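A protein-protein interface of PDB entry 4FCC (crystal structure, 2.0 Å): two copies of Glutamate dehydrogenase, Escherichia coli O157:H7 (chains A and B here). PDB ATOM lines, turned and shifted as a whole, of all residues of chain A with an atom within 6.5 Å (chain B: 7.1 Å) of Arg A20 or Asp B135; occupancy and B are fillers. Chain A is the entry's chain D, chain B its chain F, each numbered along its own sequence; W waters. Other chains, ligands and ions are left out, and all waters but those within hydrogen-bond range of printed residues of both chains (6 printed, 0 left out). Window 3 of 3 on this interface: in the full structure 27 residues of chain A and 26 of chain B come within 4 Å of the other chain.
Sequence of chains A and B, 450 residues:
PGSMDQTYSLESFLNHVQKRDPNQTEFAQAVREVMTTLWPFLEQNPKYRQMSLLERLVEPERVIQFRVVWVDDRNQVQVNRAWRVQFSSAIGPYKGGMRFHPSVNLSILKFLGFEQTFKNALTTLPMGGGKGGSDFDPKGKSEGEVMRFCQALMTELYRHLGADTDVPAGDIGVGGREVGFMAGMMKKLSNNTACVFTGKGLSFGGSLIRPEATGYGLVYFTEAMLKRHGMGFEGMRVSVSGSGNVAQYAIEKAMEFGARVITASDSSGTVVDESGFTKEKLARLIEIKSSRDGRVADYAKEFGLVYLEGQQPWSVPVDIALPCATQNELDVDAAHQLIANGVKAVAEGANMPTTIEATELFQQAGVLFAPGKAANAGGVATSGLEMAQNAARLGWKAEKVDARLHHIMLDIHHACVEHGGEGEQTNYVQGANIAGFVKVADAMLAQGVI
The side-chain carboxylate of Asp B135 is in hydrogen-bond range of the side-chain amide nitrogen of Asn B80. OE2 of Glu A55 lies within hydrogen-bond range of NE2 of His A16 (2.8 Å). The backbone carbonyl oxygen of Asn B80 is in hydrogen-bond range of the backbone NH of Val B68. ND2 of Asn B80 lies close to N of Phe B136 (3.4 Å). The backbone carbonyl oxygen (O) of Arg B81 sits at hydrogen-bond distance from the side-chain hydroxyl (OG) of Ser B134 (2.7 Å). The side-chain carboxylate of Asp A21 lies close to the side-chain amide oxygen of Gln A24.
The side-chain carboxylate of Glu A59 is in salt-bridge range of the guanidinium group of Arg B81 (2.8 Å). NH2 of Arg A20 lies within hydrogen-bond range of O of Val B79 (2.6 Å). OD2 of Asp B135 lies within salt-bridge range of NE of Arg A20 (2.6 Å). NH2 of Arg B81 lies within salt-bridge range of OD2 of Asp A21 (2.8 Å).
Among the printed residues, merely in contact across the chains: Arg A20 with Asn B80 (3.2 Å), Arg A20 with Arg B81 (3.6 Å), Glu A55 with Val B79 (3.8 Å) and Glu A59 with Gln B65 (3.8 Å).
Water W5 lies within hydrogen-bond range of OE1 of Glu A55 (2.6 Å), N of Val B79 (3.0 Å) and OE1 of Gln B78 (3.2 Å). Water W2 lies within hydrogen-bond range of the side-chain carboxylate (OE2) of Glu A59 (2.6 Å) and the side-chain amide nitrogen (NE2) of Gln B65 (2.8 Å). Water W3 lies within hydrogen-bond range of OD1 of Asp A21, OE1 of Gln B65, NH1 of Arg B81 and NE2 of Gln A24. Water W4 lies within hydrogen-bond range of O of Arg A20 (2.8 Å) and NH1 of Arg B81 (3.1 Å). Water W1 lies within hydrogen-bond range of NH2 of Arg A20 (2.9 Å) and ND2 of Asn B80 (3.4 Å). Water W6 lies within hydrogen-bond range of NH2 of Arg B81 and OE1 of Glu A59.
Asp B135 touches just one residue of chain A: Arg A20. Of the printed residues of chain A, Gln B65 touches Glu A59. Of the printed residues of chain A, Arg B81 touches Arg A20, Asp A21 and Glu A59. Of the printed residues of chain B, Glu A59 touches Gln B65 and Arg B81. Of the printed residues of chain B, Glu A55 touches Val B79 (3.8 Å). Of the printed residues of chain A, Val B79 touches Arg A20 (2.6 Å) and Glu A55 (3.8 Å). The nearest residue of chain B that does not touch Arg A20 is Asn B105 (6.0 Å). The nearest printed residue of chain A that does not touch Asp B135 is Glu A59 (6.8 Å).
Hydrophobic or aromatic side chains of chain B that line the printed part of chain A: Val B79. Along chain B the printed residues that touch a printed residue of chain A span positions 65 to 135. Of the 12 printed residues of chain A, 4 touch a printed residue of chain B. Among the printed residues, 8 pairs touch across the chains. Among the printed residues, Asp or Glu carboxylates within 4 Å of a Lys or Arg side-chain nitrogen of the other chain: Arg A20 with Asp B135 (2.6 Å), Asp A21 with Arg B81 (2.8 Å) and Glu A59 with Arg B81 (2.8 Å).
No position is printed for both chains.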
ATOM      1  N   ASN A  15      11.472  12.981 -20.414  1.00  0.00           N
ATOM      2  CA  ASN A  15      11.697  11.715 -21.086  1.00  0.00           C
ATOM      3  C   ASN A  15      13.184  11.382 -21.119  1.00  0.00           C
ATOM      4  O   ASN A  15      13.581  10.253 -20.834  1.00  0.00           O
ATOM      5  CB  ASN A  15      11.109  11.762 -22.500  1.00  0.00           C
ATOM      6  CG  ASN A  15      11.686  10.696 -23.406  1.00  0.00           C
ATOM      7  OD1 ASN A  15      12.751  10.881 -24.000  1.00  0.00           O
ATOM      8  ND2 ASN A  15      10.989   9.572 -23.516  1.00  0.00           N
ATOM      9  N   HIS A  16      14.002  12.379 -21.441  1.00  0.00           N
ATOM     10  CA  HIS A  16      15.448  12.197 -21.500  1.00  0.00           C
ATOM     11  C   HIS A  16      16.023  11.748 -20.159  1.00  0.00           C
ATOM     12  O   HIS A  16      16.864  10.849 -20.105  1.00  0.00           O
ATOM     13  CB  HIS A  16      16.134  13.488 -21.953  1.00  0.00           C
ATOM     14  CG  HIS A  16      17.616  13.496 -21.733  1.00  0.00           C
ATOM     15  ND1 HIS A  16      18.475  12.657 -22.408  1.00  0.00           N
ATOM     16  CD2 HIS A  16      18.390  14.243 -20.909  1.00  0.00           C
ATOM     17  CE1 HIS A  16      19.714  12.887 -22.012  1.00  0.00           C
ATOM     18  NE2 HIS A  16      19.692  13.844 -21.103  1.00  0.00           N
ATOM     19  N   VAL A  17      15.569  12.364 -19.073  1.00  0.00           N
ATOM     20  CA  VAL A  17      16.115  12.021 -17.759  1.00  0.00           C
ATOM     21  C   VAL A  17      15.595  10.676 -17.247  1.00  0.00           C
ATOM     22  O   VAL A  17      16.324   9.942 -16.587  1.00  0.00           O
ATOM     23  CB  VAL A  17      15.906  13.144 -16.704  1.00  0.00           C
ATOM     24  CG1 VAL A  17      16.660  14.402 -17.108  1.00  0.00           C
ATOM     25  CG2 VAL A  17      14.441  13.445 -16.521  1.00  0.00           C
ATOM     26  N   GLN A  18      14.351  10.338 -17.576  1.00  0.00           N
ATOM     27  CA  GLN A  18      13.801   9.036 -17.189  1.00  0.00           C
ATOM     28  C   GLN A  18      14.541   7.844 -17.829  1.00  0.00           C
ATOM     29  O   GLN A  18      14.500   6.736 -17.304  1.00  0.00           O
ATOM     30  CB  GLN A  18      12.296   8.951 -17.491  1.00  0.00           C
ATOM     31  CG  GLN A  18      11.638   7.715 -16.892  1.00  0.00           C
ATOM     32  CD  GLN A  18      10.133   7.693 -17.049  1.00  0.00           C
ATOM     33  OE1 GLN A  18       9.593   8.131 -18.063  1.00  0.00           O
ATOM     34  NE2 GLN A  18       9.444   7.179 -16.038  1.00  0.00           N
ATOM     35  N   LYS A  19      15.211   8.073 -18.955  1.00  0.00           N
ATOM     36  CA  LYS A  19      15.975   7.013 -19.622  1.00  0.00           C
ATOM     37  C   LYS A  19      16.962   6.279 -18.705  1.00  0.00           C
ATOM     38  O   LYS A  19      17.117   5.066 -18.813  1.00  0.00           O
ATOM     39  CB  LYS A  19      16.710   7.557 -20.851  1.00  0.00           C
ATOM     40  CG  LYS A  19      15.796   8.178 -21.887  1.00  0.00           C
ATOM     41  CD  LYS A  19      16.130   7.681 -23.284  1.00  0.00           C
ATOM     42  CE  LYS A  19      15.179   8.272 -24.321  1.00  0.00           C
ATOM     43  NZ  LYS A  19      15.437   7.729 -25.690  1.00  0.00           N
ATOM     44  N   ARG A  20      17.621   7.008 -17.807  1.00  0.00           N
ATOM     45  CA  ARG A  20      18.551   6.386 -16.865  1.00  0.00           C
ATOM     46  C   ARG A  20      17.849   5.587 -15.769  1.00  0.00           C
ATOM     47  O   ARG A  20      18.423   4.658 -15.202  1.00  0.00           O
ATOM     48  CB  ARG A  20      19.475   7.432 -16.221  1.00  0.00           C
ATOM     49  CG  ARG A  20      20.656   7.833 -17.098  1.00  0.00           C
ATOM     50  CD  ARG A  20      21.749   8.612 -16.335  1.00  0.00           C
ATOM     51  NE  ARG A  20      22.735   9.106 -17.297  1.00  0.00           N
ATOM     52  CZ  ARG A  20      23.008  10.387 -17.515  1.00  0.00           C
ATOM     53  NH1 ARG A  20      22.408  11.333 -16.807  1.00  0.00           N
ATOM     54  NH2 ARG A  20      23.896  10.721 -18.437  1.00  0.00           N
ATOM     55  N   ASP A  21      16.613   5.959 -15.462  1.00  0.00           N
ATOM     56  CA  ASP A  21      15.892   5.345 -14.354  1.00  0.00           C
ATOM     57  C   ASP A  21      14.463   5.028 -14.763  1.00  0.00           C
ATOM     58  O   ASP A  21      13.519   5.552 -14.174  1.00  0.00           O
ATOM     59  CB  ASP A  21      15.883   6.286 -13.139  1.00  0.00           C
ATOM     60  CG  ASP A  21      17.278   6.575 -12.604  1.00  0.00           C
ATOM     61  OD1 ASP A  21      17.958   5.630 -12.140  1.00  0.00           O
ATOM     62  OD2 ASP A  21      17.686   7.756 -12.624  1.00  0.00           O
ATOM     63  N   PRO A  22      14.298   4.148 -15.764  1.00  0.00           N
ATOM     64  CA  PRO A  22      12.981   3.951 -16.380  1.00  0.00           C
ATOM     65  C   PRO A  22      11.954   3.343 -15.426  1.00  0.00           C
ATOM     66  O   PRO A  22      10.759   3.440 -15.699  1.00  0.00           O
ATOM     67  CB  PRO A  22      13.280   3.000 -17.543  1.00  0.00           C
ATOM     68  CG  PRO A  22      14.485   2.230 -17.089  1.00  0.00           C
ATOM     69  CD  PRO A  22      15.305   3.212 -16.299  1.00  0.00           C
ATOM     70  N   ASN A  23      12.400   2.742 -14.326  1.00  0.00           N
ATOM     71  CA  ASN A  23      11.468   2.142 -13.373  1.00  0.00           C
ATOM     72  C   ASN A  23      11.390   2.867 -12.020  1.00  0.00           C
ATOM     73  O   ASN A  23      10.750   2.381 -11.085  1.00  0.00           O
ATOM     74  CB  ASN A  23      11.772   0.649 -13.176  1.00  0.00           C
ATOM     75  CG  ASN A  23      11.616  -0.151 -14.457  1.00  0.00           C
ATOM     76  OD1 ASN A  23      12.592  -0.659 -15.011  1.00  0.00           O
ATOM     77  ND2 ASN A  23      10.378  -0.270 -14.933  1.00  0.00           N
ATOM     78  N   GLN A  24      12.041   4.024 -11.916  1.00  0.00           N
ATOM     79  CA  GLN A  24      11.957   4.826 -10.696  1.00  0.00           C
ATOM     80  C   GLN A  24      10.742   5.739 -10.809  1.00  0.00           C
ATOM     81  O   GLN A  24      10.850   6.892 -11.232  1.00  0.00           O
ATOM     82  CB  GLN A  24      13.244   5.626 -10.450  1.00  0.00           C
ATOM     83  CG  GLN A  24      14.438   4.755 -10.081  1.00  0.00           C
ATOM     84  CD  GLN A  24      15.708   5.537  -9.759  1.00  0.00           C
ATOM     85  OE1 GLN A  24      15.822   6.726 -10.055  1.00  0.00           O
ATOM     86  NE2 GLN A  24      16.678   4.855  -9.164  1.00  0.00           N
ATOM     87  N   GLU A  55      19.966  18.968 -15.835  1.00  0.00           N
ATOM     88  CA  GLU A  55      20.598  17.656 -15.837  1.00  0.00           C
ATOM     89  C   GLU A  55      21.519  17.455 -14.638  1.00  0.00           C
ATOM     90  O   GLU A  55      21.525  16.382 -14.025  1.00  0.00           O
ATOM     91  CB  GLU A  55      21.422  17.462 -17.101  1.00  0.00           C
ATOM     92  CG  GLU A  55      20.655  16.948 -18.302  1.00  0.00           C
ATOM     93  CD  GLU A  55      21.597  16.365 -19.329  1.00  0.00           C
ATOM     94  OE1 GLU A  55      22.343  17.147 -19.956  1.00  0.00           O
ATOM     95  OE2 GLU A  55      21.623  15.125 -19.481  1.00  0.00           O
ATOM     96  N   GLU A  59      20.664  14.675 -11.265  1.00  0.00           N
ATOM     97  CA  GLU A  59      21.592  13.573 -11.050  1.00  0.00           C
ATOM     98  C   GLU A  59      22.309  13.765  -9.718  1.00  0.00           C
ATOM     99  O   GLU A  59      23.112  14.693  -9.568  1.00  0.00           O
ATOM    100  CB  GLU A  59      22.595  13.492 -12.197  1.00  0.00           C
ATOM    101  CG  GLU A  59      23.603  12.341 -12.097  1.00  0.00           C
ATOM    102  CD  GLU A  59      22.984  10.966 -12.309  1.00  0.00           C
ATOM    103  OE1 GLU A  59      21.842  10.883 -12.812  1.00  0.00           O
ATOM    104  OE2 GLU A  59      23.644   9.963 -11.966  1.00  0.00           O
ATOM    105  N   GLN B  65      27.219   4.886  -6.869  1.00  0.00           N
ATOM    106  CA  GLN B  65      26.737   5.532  -8.088  1.00  0.00           C
ATOM    107  C   GLN B  65      27.048   7.006  -7.936  1.00  0.00           C
ATOM    108  O   GLN B  65      26.810   7.593  -6.872  1.00  0.00           O
ATOM    109  CB  GLN B  65      25.226   5.338  -8.285  1.00  0.00           C
ATOM    110  CG  GLN B  65      24.669   6.090  -9.506  1.00  0.00           C
ATOM    111  CD  GLN B  65      23.155   6.301  -9.449  1.00  0.00           C
ATOM    112  OE1 GLN B  65      22.381   5.374  -9.674  1.00  0.00           O
ATOM    113  NE2 GLN B  65      22.734   7.534  -9.159  1.00  0.00           N
ATOM    114  N   VAL B  68      28.915  12.375 -13.087  1.00  0.00           N
ATOM    115  CA  VAL B  68      30.139  12.839 -13.725  1.00  0.00           C
ATOM    116  C   VAL B  68      29.847  14.020 -14.641  1.00  0.00           C
ATOM    117  O   VAL B  68      29.112  13.885 -15.643  1.00  0.00           O
ATOM    118  CB  VAL B  68      30.848  11.701 -14.519  1.00  0.00           C
ATOM    119  CG1 VAL B  68      32.115  12.224 -15.186  1.00  0.00           C
ATOM    120  CG2 VAL B  68      31.195  10.533 -13.591  1.00  0.00           C
ATOM    121  N   GLN B  78      28.190  18.386 -20.252  1.00  0.00           N
ATOM    122  CA  GLN B  78      27.525  17.093 -20.361  1.00  0.00           C
ATOM    123  C   GLN B  78      27.464  16.410 -18.997  1.00  0.00           C
ATOM    124  O   GLN B  78      28.361  16.577 -18.172  1.00  0.00           O
ATOM    125  CB  GLN B  78      28.270  16.190 -21.341  1.00  0.00           C
ATOM    126  CG  GLN B  78      28.428  16.772 -22.750  1.00  0.00           C
ATOM    127  CD  GLN B  78      27.098  16.975 -23.464  1.00  0.00           C
ATOM    128  OE1 GLN B  78      26.093  16.347 -23.125  1.00  0.00           O
ATOM    129  NE2 GLN B  78      27.086  17.867 -24.449  1.00  0.00           N
ATOM    130  N   VAL B  79      26.406  15.638 -18.768  1.00  0.00           N
ATOM    131  CA  VAL B  79      26.247  14.924 -17.517  1.00  0.00           C
ATOM    132  C   VAL B  79      26.117  13.427 -17.767  1.00  0.00           C
ATOM    133  O   VAL B  79      25.233  12.994 -18.501  1.00  0.00           O
ATOM    134  CB  VAL B  79      25.014  15.409 -16.742  1.00  0.00           C
ATOM    135  CG1 VAL B  79      24.902  14.659 -15.422  1.00  0.00           C
ATOM    136  CG2 VAL B  79      25.103  16.898 -16.486  1.00  0.00           C
ATOM    137  N   ASN B  80      26.993  12.635 -17.152  1.00  0.00           N
ATOM    138  CA  ASN B  80      26.885  11.185 -17.261  1.00  0.00           C
ATOM    139  C   ASN B  80      26.822  10.514 -15.900  1.00  0.00           C
ATOM    140  O   ASN B  80      27.208  11.098 -14.887  1.00  0.00           O
ATOM    141  CB  ASN B  80      28.038  10.599 -18.089  1.00  0.00           C
ATOM    142  CG  ASN B  80      27.872  10.860 -19.584  1.00  0.00           C
ATOM    143  OD1 ASN B  80      28.417  11.824 -20.107  1.00  0.00           O
ATOM    144  ND2 ASN B  80      27.096  10.014 -20.266  1.00  0.00           N
ATOM    145  N   ARG B  81      26.334   9.284 -15.878  1.00  0.00           N
ATOM    146  CA  ARG B  81      26.317   8.507 -14.651  1.00  0.00           C
ATOM    147  C   ARG B  81      27.474   7.518 -14.672  1.00  0.00           C
ATOM    148  O   ARG B  81      27.808   6.973 -15.733  1.00  0.00           O
ATOM    149  CB  ARG B  81      24.996   7.764 -14.509  1.00  0.00           C
ATOM    150  CG  ARG B  81      24.898   6.936 -13.259  1.00  0.00           C
ATOM    151  CD  ARG B  81      23.487   6.447 -13.067  1.00  0.00           C
ATOM    152  NE  ARG B  81      22.542   7.525 -12.801  1.00  0.00           N
ATOM    153  CZ  ARG B  81      21.238   7.330 -12.668  1.00  0.00           C
ATOM    154  NH1 ARG B  81      20.750   6.099 -12.791  1.00  0.00           N
ATOM    155  NH2 ARG B  81      20.426   8.355 -12.421  1.00  0.00           N
ATOM    156  N   ALA B  82      28.096   7.312 -13.510  1.00  0.00           N
ATOM    157  CA  ALA B  82      29.110   6.269 -13.354  1.00  0.00           C
ATOM    158  C   ALA B  82      28.885   5.458 -12.081  1.00  0.00           C
ATOM    159  O   ALA B  82      28.151   5.878 -11.189  1.00  0.00           O
ATOM    160  CB  ALA B  82      30.519   6.866 -13.374  1.00  0.00           C
ATOM    161  N   TRP B  83      29.512   4.285 -12.011  1.00  0.00           N
ATOM    162  CA  TRP B  83      29.361   3.422 -10.856  1.00  0.00           C
ATOM    163  C   TRP B  83      30.673   2.747 -10.536  1.00  0.00           C
ATOM    164  O   TRP B  83      31.521   2.577 -11.410  1.00  0.00           O
ATOM    165  CB  TRP B  83      28.411   2.268 -11.134  1.00  0.00           C
ATOM    166  CG  TRP B  83      27.023   2.558 -11.509  1.00  0.00           C
ATOM    167  CD1 TRP B  83      25.920   2.444 -10.713  1.00  0.00           C
ATOM    168  CD2 TRP B  83      26.552   2.922 -12.805  1.00  0.00           C
ATOM    169  NE1 TRP B  83      24.788   2.752 -11.434  1.00  0.00           N
ATOM    170  CE2 TRP B  83      25.152   3.042 -12.723  1.00  0.00           C
ATOM    171  CE3 TRP B  83      27.180   3.164 -14.031  1.00  0.00           C
ATOM    172  CZ2 TRP B  83      24.369   3.390 -13.819  1.00  0.00           C
ATOM    173  CZ3 TRP B  83      26.393   3.521 -15.120  1.00  0.00           C
ATOM    174  CH2 TRP B  83      25.011   3.638 -14.999  1.00  0.00           C
ATOM    175  N   ARG B  99      33.915  -0.122 -17.566  1.00  0.00           N
ATOM    176  CA  ARG B  99      33.326  -0.206 -18.909  1.00  0.00           C
ATOM    177  C   ARG B  99      32.598   1.087 -19.288  1.00  0.00           C
ATOM    178  O   ARG B  99      31.679   1.512 -18.595  1.00  0.00           O
ATOM    179  CB  ARG B  99      32.363  -1.397 -18.982  1.00  0.00           C
ATOM    180  CG  ARG B  99      31.589  -1.502 -20.284  1.00  0.00           C
ATOM    181  CD  ARG B  99      30.682  -2.726 -20.301  1.00  0.00           C
ATOM    182  NE  ARG B  99      31.432  -3.981 -20.256  1.00  0.00           N
ATOM    183  CZ  ARG B  99      30.908  -5.171 -20.535  1.00  0.00           C
ATOM    184  NH1 ARG B  99      29.624  -5.276 -20.884  1.00  0.00           N
ATOM    185  NH2 ARG B  99      31.665  -6.259 -20.473  1.00  0.00           N
ATOM    186  N   PHE B 100      33.017   1.714 -20.386  1.00  0.00           N
ATOM    187  CA  PHE B 100      32.349   2.909 -20.870  1.00  0.00           C
ATOM    188  C   PHE B 100      31.489   2.539 -22.093  1.00  0.00           C
ATOM    189  O   PHE B 100      32.015   2.335 -23.176  1.00  0.00           O
ATOM    190  CB  PHE B 100      33.369   3.975 -21.275  1.00  0.00           C
ATOM    191  CG  PHE B 100      34.215   4.497 -20.138  1.00  0.00           C
ATOM    192  CD1 PHE B 100      33.978   4.114 -18.821  1.00  0.00           C
ATOM    193  CD2 PHE B 100      35.266   5.363 -20.399  1.00  0.00           C
ATOM    194  CE1 PHE B 100      34.775   4.594 -17.777  1.00  0.00           C
ATOM    195  CE2 PHE B 100      36.068   5.835 -19.366  1.00  0.00           C
ATOM    196  CZ  PHE B 100      35.805   5.461 -18.050  1.00  0.00           C
ATOM    197  N   HIS B 101      30.176   2.440 -21.911  1.00  0.00           N
ATOM    198  CA  HIS B 101      29.270   2.158 -23.038  1.00  0.00           C
ATOM    199  C   HIS B 101      27.874   2.687 -22.705  1.00  0.00           C
ATOM    200  O   HIS B 101      27.457   2.631 -21.547  1.00  0.00           O
ATOM    201  CB  HIS B 101      29.230   0.657 -23.340  1.00  0.00           C
ATOM    202  CG  HIS B 101      28.493   0.304 -24.594  1.00  0.00           C
ATOM    203  ND1 HIS B 101      27.125   0.145 -24.633  1.00  0.00           N
ATOM    204  CD2 HIS B 101      28.931   0.090 -25.859  1.00  0.00           C
ATOM    205  CE1 HIS B 101      26.749  -0.155 -25.864  1.00  0.00           C
ATOM    206  NE2 HIS B 101      27.826  -0.193 -26.629  1.00  0.00           N
ATOM    207  N   PRO B 102      27.151   3.225 -23.708  1.00  0.00           N
ATOM    208  CA  PRO B 102      25.811   3.774 -23.440  1.00  0.00           C
ATOM    209  C   PRO B 102      24.819   2.763 -22.854  1.00  0.00           C
ATOM    210  O   PRO B 102      23.806   3.182 -22.311  1.00  0.00           O
ATOM    211  CB  PRO B 102      25.331   4.236 -24.832  1.00  0.00           C
ATOM    212  CG  PRO B 102      26.209   3.494 -25.815  1.00  0.00           C
ATOM    213  CD  PRO B 102      27.544   3.420 -25.113  1.00  0.00           C
ATOM    214  N   SER B 103      25.101   1.467 -22.970  1.00  0.00           N
ATOM    215  CA  SER B 103      24.211   0.423 -22.461  1.00  0.00           C
ATOM    216  C   SER B 103      24.451   0.096 -20.986  1.00  0.00           C
ATOM    217  O   SER B 103      23.617  -0.546 -20.349  1.00  0.00           O
ATOM    218  CB  SER B 103      24.384  -0.852 -23.278  1.00  0.00           C
ATOM    219  OG  SER B 103      25.681  -1.384 -23.071  1.00  0.00           O
ATOM    220  N   VAL B 104      25.598   0.534 -20.463  1.00  0.00           N
ATOM    221  CA  VAL B 104      25.987   0.294 -19.072  1.00  0.00           C
ATOM    222  C   VAL B 104      24.921   0.755 -18.079  1.00  0.00           C
ATOM    223  O   VAL B 104      24.386   1.852 -18.194  1.00  0.00           O
ATOM    224  CB  VAL B 104      27.341   0.979 -18.762  1.00  0.00           C
ATOM    225  CG1 VAL B 104      27.717   0.842 -17.300  1.00  0.00           C
ATOM    226  CG2 VAL B 104      28.430   0.379 -19.626  1.00  0.00           C
ATOM    227  N   ASN B 105      24.586  -0.116 -17.131  1.00  0.00           N
ATOM    228  CA  ASN B 105      23.700   0.240 -16.029  1.00  0.00           C
ATOM    229  C   ASN B 105      24.040  -0.618 -14.826  1.00  0.00           C
ATOM    230  O   ASN B 105      24.958  -1.436 -14.893  1.00  0.00           O
ATOM    231  CB  ASN B 105      22.209   0.141 -16.421  1.00  0.00           C
ATOM    232  CG  ASN B 105      21.794  -1.255 -16.871  1.00  0.00           C
ATOM    233  OD1 ASN B 105      22.300  -2.256 -16.379  1.00  0.00           O
ATOM    234  ND2 ASN B 105      20.860  -1.318 -17.819  1.00  0.00           N
ATOM    235  N   GLY B 133      32.048   1.479 -14.276  1.00  0.00           N
ATOM    236  CA  GLY B 133      31.869   1.998 -15.618  1.00  0.00           C
ATOM    237  C   GLY B 133      30.919   3.171 -15.650  1.00  0.00           C
ATOM    238  O   GLY B 133      30.647   3.773 -14.617  1.00  0.00           O
ATOM    239  N   SER B 134      30.414   3.483 -16.838  1.00  0.00           N
ATOM    240  CA  SER B 134      29.655   4.709 -17.059  1.00  0.00           C
ATOM    241  C   SER B 134      28.870   4.615 -18.367  1.00  0.00           C
ATOM    242  O   SER B 134      29.277   3.884 -19.272  1.00  0.00           O
ATOM    243  CB  SER B 134      30.618   5.895 -17.128  1.00  0.00           C
ATOM    244  OG  SER B 134      29.939   7.096 -17.449  1.00  0.00           O
ATOM    245  N   ASP B 135      27.758   5.349 -18.473  1.00  0.00           N
ATOM    246  CA  ASP B 135      26.981   5.366 -19.717  1.00  0.00           C
ATOM    247  C   ASP B 135      27.594   6.309 -20.748  1.00  0.00           C
ATOM    248  O   ASP B 135      27.078   6.440 -21.844  1.00  0.00           O
ATOM    249  CB  ASP B 135      25.489   5.690 -19.490  1.00  0.00           C
ATOM    250  CG  ASP B 135      25.272   6.922 -18.625  1.00  0.00           C
ATOM    251  OD1 ASP B 135      26.204   7.741 -18.487  1.00  0.00           O
ATOM    252  OD2 ASP B 135      24.159   7.063 -18.072  1.00  0.00           O
ATOM    253  N   PHE B 136      28.690   6.963 -20.373  1.00  0.00           N
ATOM    254  CA  PHE B 136      29.531   7.710 -21.307  1.00  0.00           C
ATOM    255  C   PHE B 136      29.816   6.855 -22.542  1.00  0.00           C
ATOM    256  O   PHE B 136      30.186   5.682 -22.428  1.00  0.00           O
ATOM    257  CB  PHE B 136      30.851   8.080 -20.612  1.00  0.00           C
ATOM    258  CG  PHE B 136      31.853   8.779 -21.498  1.00  0.00           C
ATOM    259  CD1 PHE B 136      31.731  10.133 -21.776  1.00  0.00           C
ATOM    260  CD2 PHE B 136      32.942   8.091 -22.017  1.00  0.00           C
ATOM    261  CE1 PHE B 136      32.663  10.788 -22.573  1.00  0.00           C
ATOM    262  CE2 PHE B 136      33.875   8.739 -22.825  1.00  0.00           C
ATOM    263  CZ  PHE B 136      33.733  10.084 -23.096  1.00  0.00           C
ATOM    264  N   ASP B 137      29.617   7.441 -23.717  1.00  0.00           N
ATOM    265  CA  ASP B 137      29.869   6.739 -24.969  1.00  0.00           C
ATOM    266  C   ASP B 137      31.140   7.275 -25.625  1.00  0.00           C
ATOM    267  O   ASP B 137      31.165   8.401 -26.102  1.00  0.00           O
ATOM    268  CB  ASP B 137      28.658   6.882 -25.895  1.00  0.00           C
ATOM    269  CG  ASP B 137      28.818   6.110 -27.192  1.00  0.00           C
ATOM    270  OD1 ASP B 137      29.805   5.352 -27.322  1.00  0.00           O
ATOM    271  OD2 ASP B 137      27.944   6.261 -28.074  1.00  0.00           O
ATOM    272  N   PRO B 138      32.211   6.464 -25.634  1.00  0.00           N
ATOM    273  CA  PRO B 138      33.507   6.838 -26.219  1.00  0.00           C
ATOM    274  C   PRO B 138      33.484   7.033 -27.748  1.00  0.00           C
ATOM    275  O   PRO B 138      34.346   7.736 -28.277  1.00  0.00           O
ATOM    276  CB  PRO B 138      34.410   5.649 -25.859  1.00  0.00           C
ATOM    277  CG  PRO B 138      33.718   4.971 -24.703  1.00  0.00           C
ATOM    278  CD  PRO B 138      32.258   5.133 -25.006  1.00  0.00           C
ATOM    279  N   PHE B 149      36.767  13.438 -19.601  1.00  0.00           N
ATOM    280  CA  PHE B 149      35.800  12.566 -18.955  1.00  0.00           C
ATOM    281  C   PHE B 149      36.437  11.692 -17.879  1.00  0.00           C
ATOM    282  O   PHE B 149      35.896  11.566 -16.783  1.00  0.00           O
ATOM    283  CB  PHE B 149      35.089  11.639 -19.922  1.00  0.00           C
ATOM    284  CG  PHE B 149      34.141  10.716 -19.223  1.00  0.00           C
ATOM    285  CD1 PHE B 149      32.941  11.203 -18.715  1.00  0.00           C
ATOM    286  CD2 PHE B 149      34.465   9.388 -19.008  1.00  0.00           C
ATOM    287  CE1 PHE B 149      32.067  10.374 -18.039  1.00  0.00           C
ATOM    288  CE2 PHE B 149      33.589   8.549 -18.323  1.00  0.00           C
ATOM    289  CZ  PHE B 149      32.386   9.050 -17.839  1.00  0.00           C
HETATM  290  O   HOH W   1      23.875   9.521 -21.120  1.00  0.00           O
HETATM  291  O   HOH W   2      24.700   9.502  -9.669  1.00  0.00           O
HETATM  292  O   HOH W   3      19.606   5.891  -9.922  1.00  0.00           O
HETATM  293  O   HOH W   4      21.194   4.193 -15.258  1.00  0.00           O
HETATM  294  O   HOH W   5      24.154  15.511 -20.703  1.00  0.00           O
HETATM  295  O   HOH W   6      18.662  10.999 -11.419  1.00  0.00           O
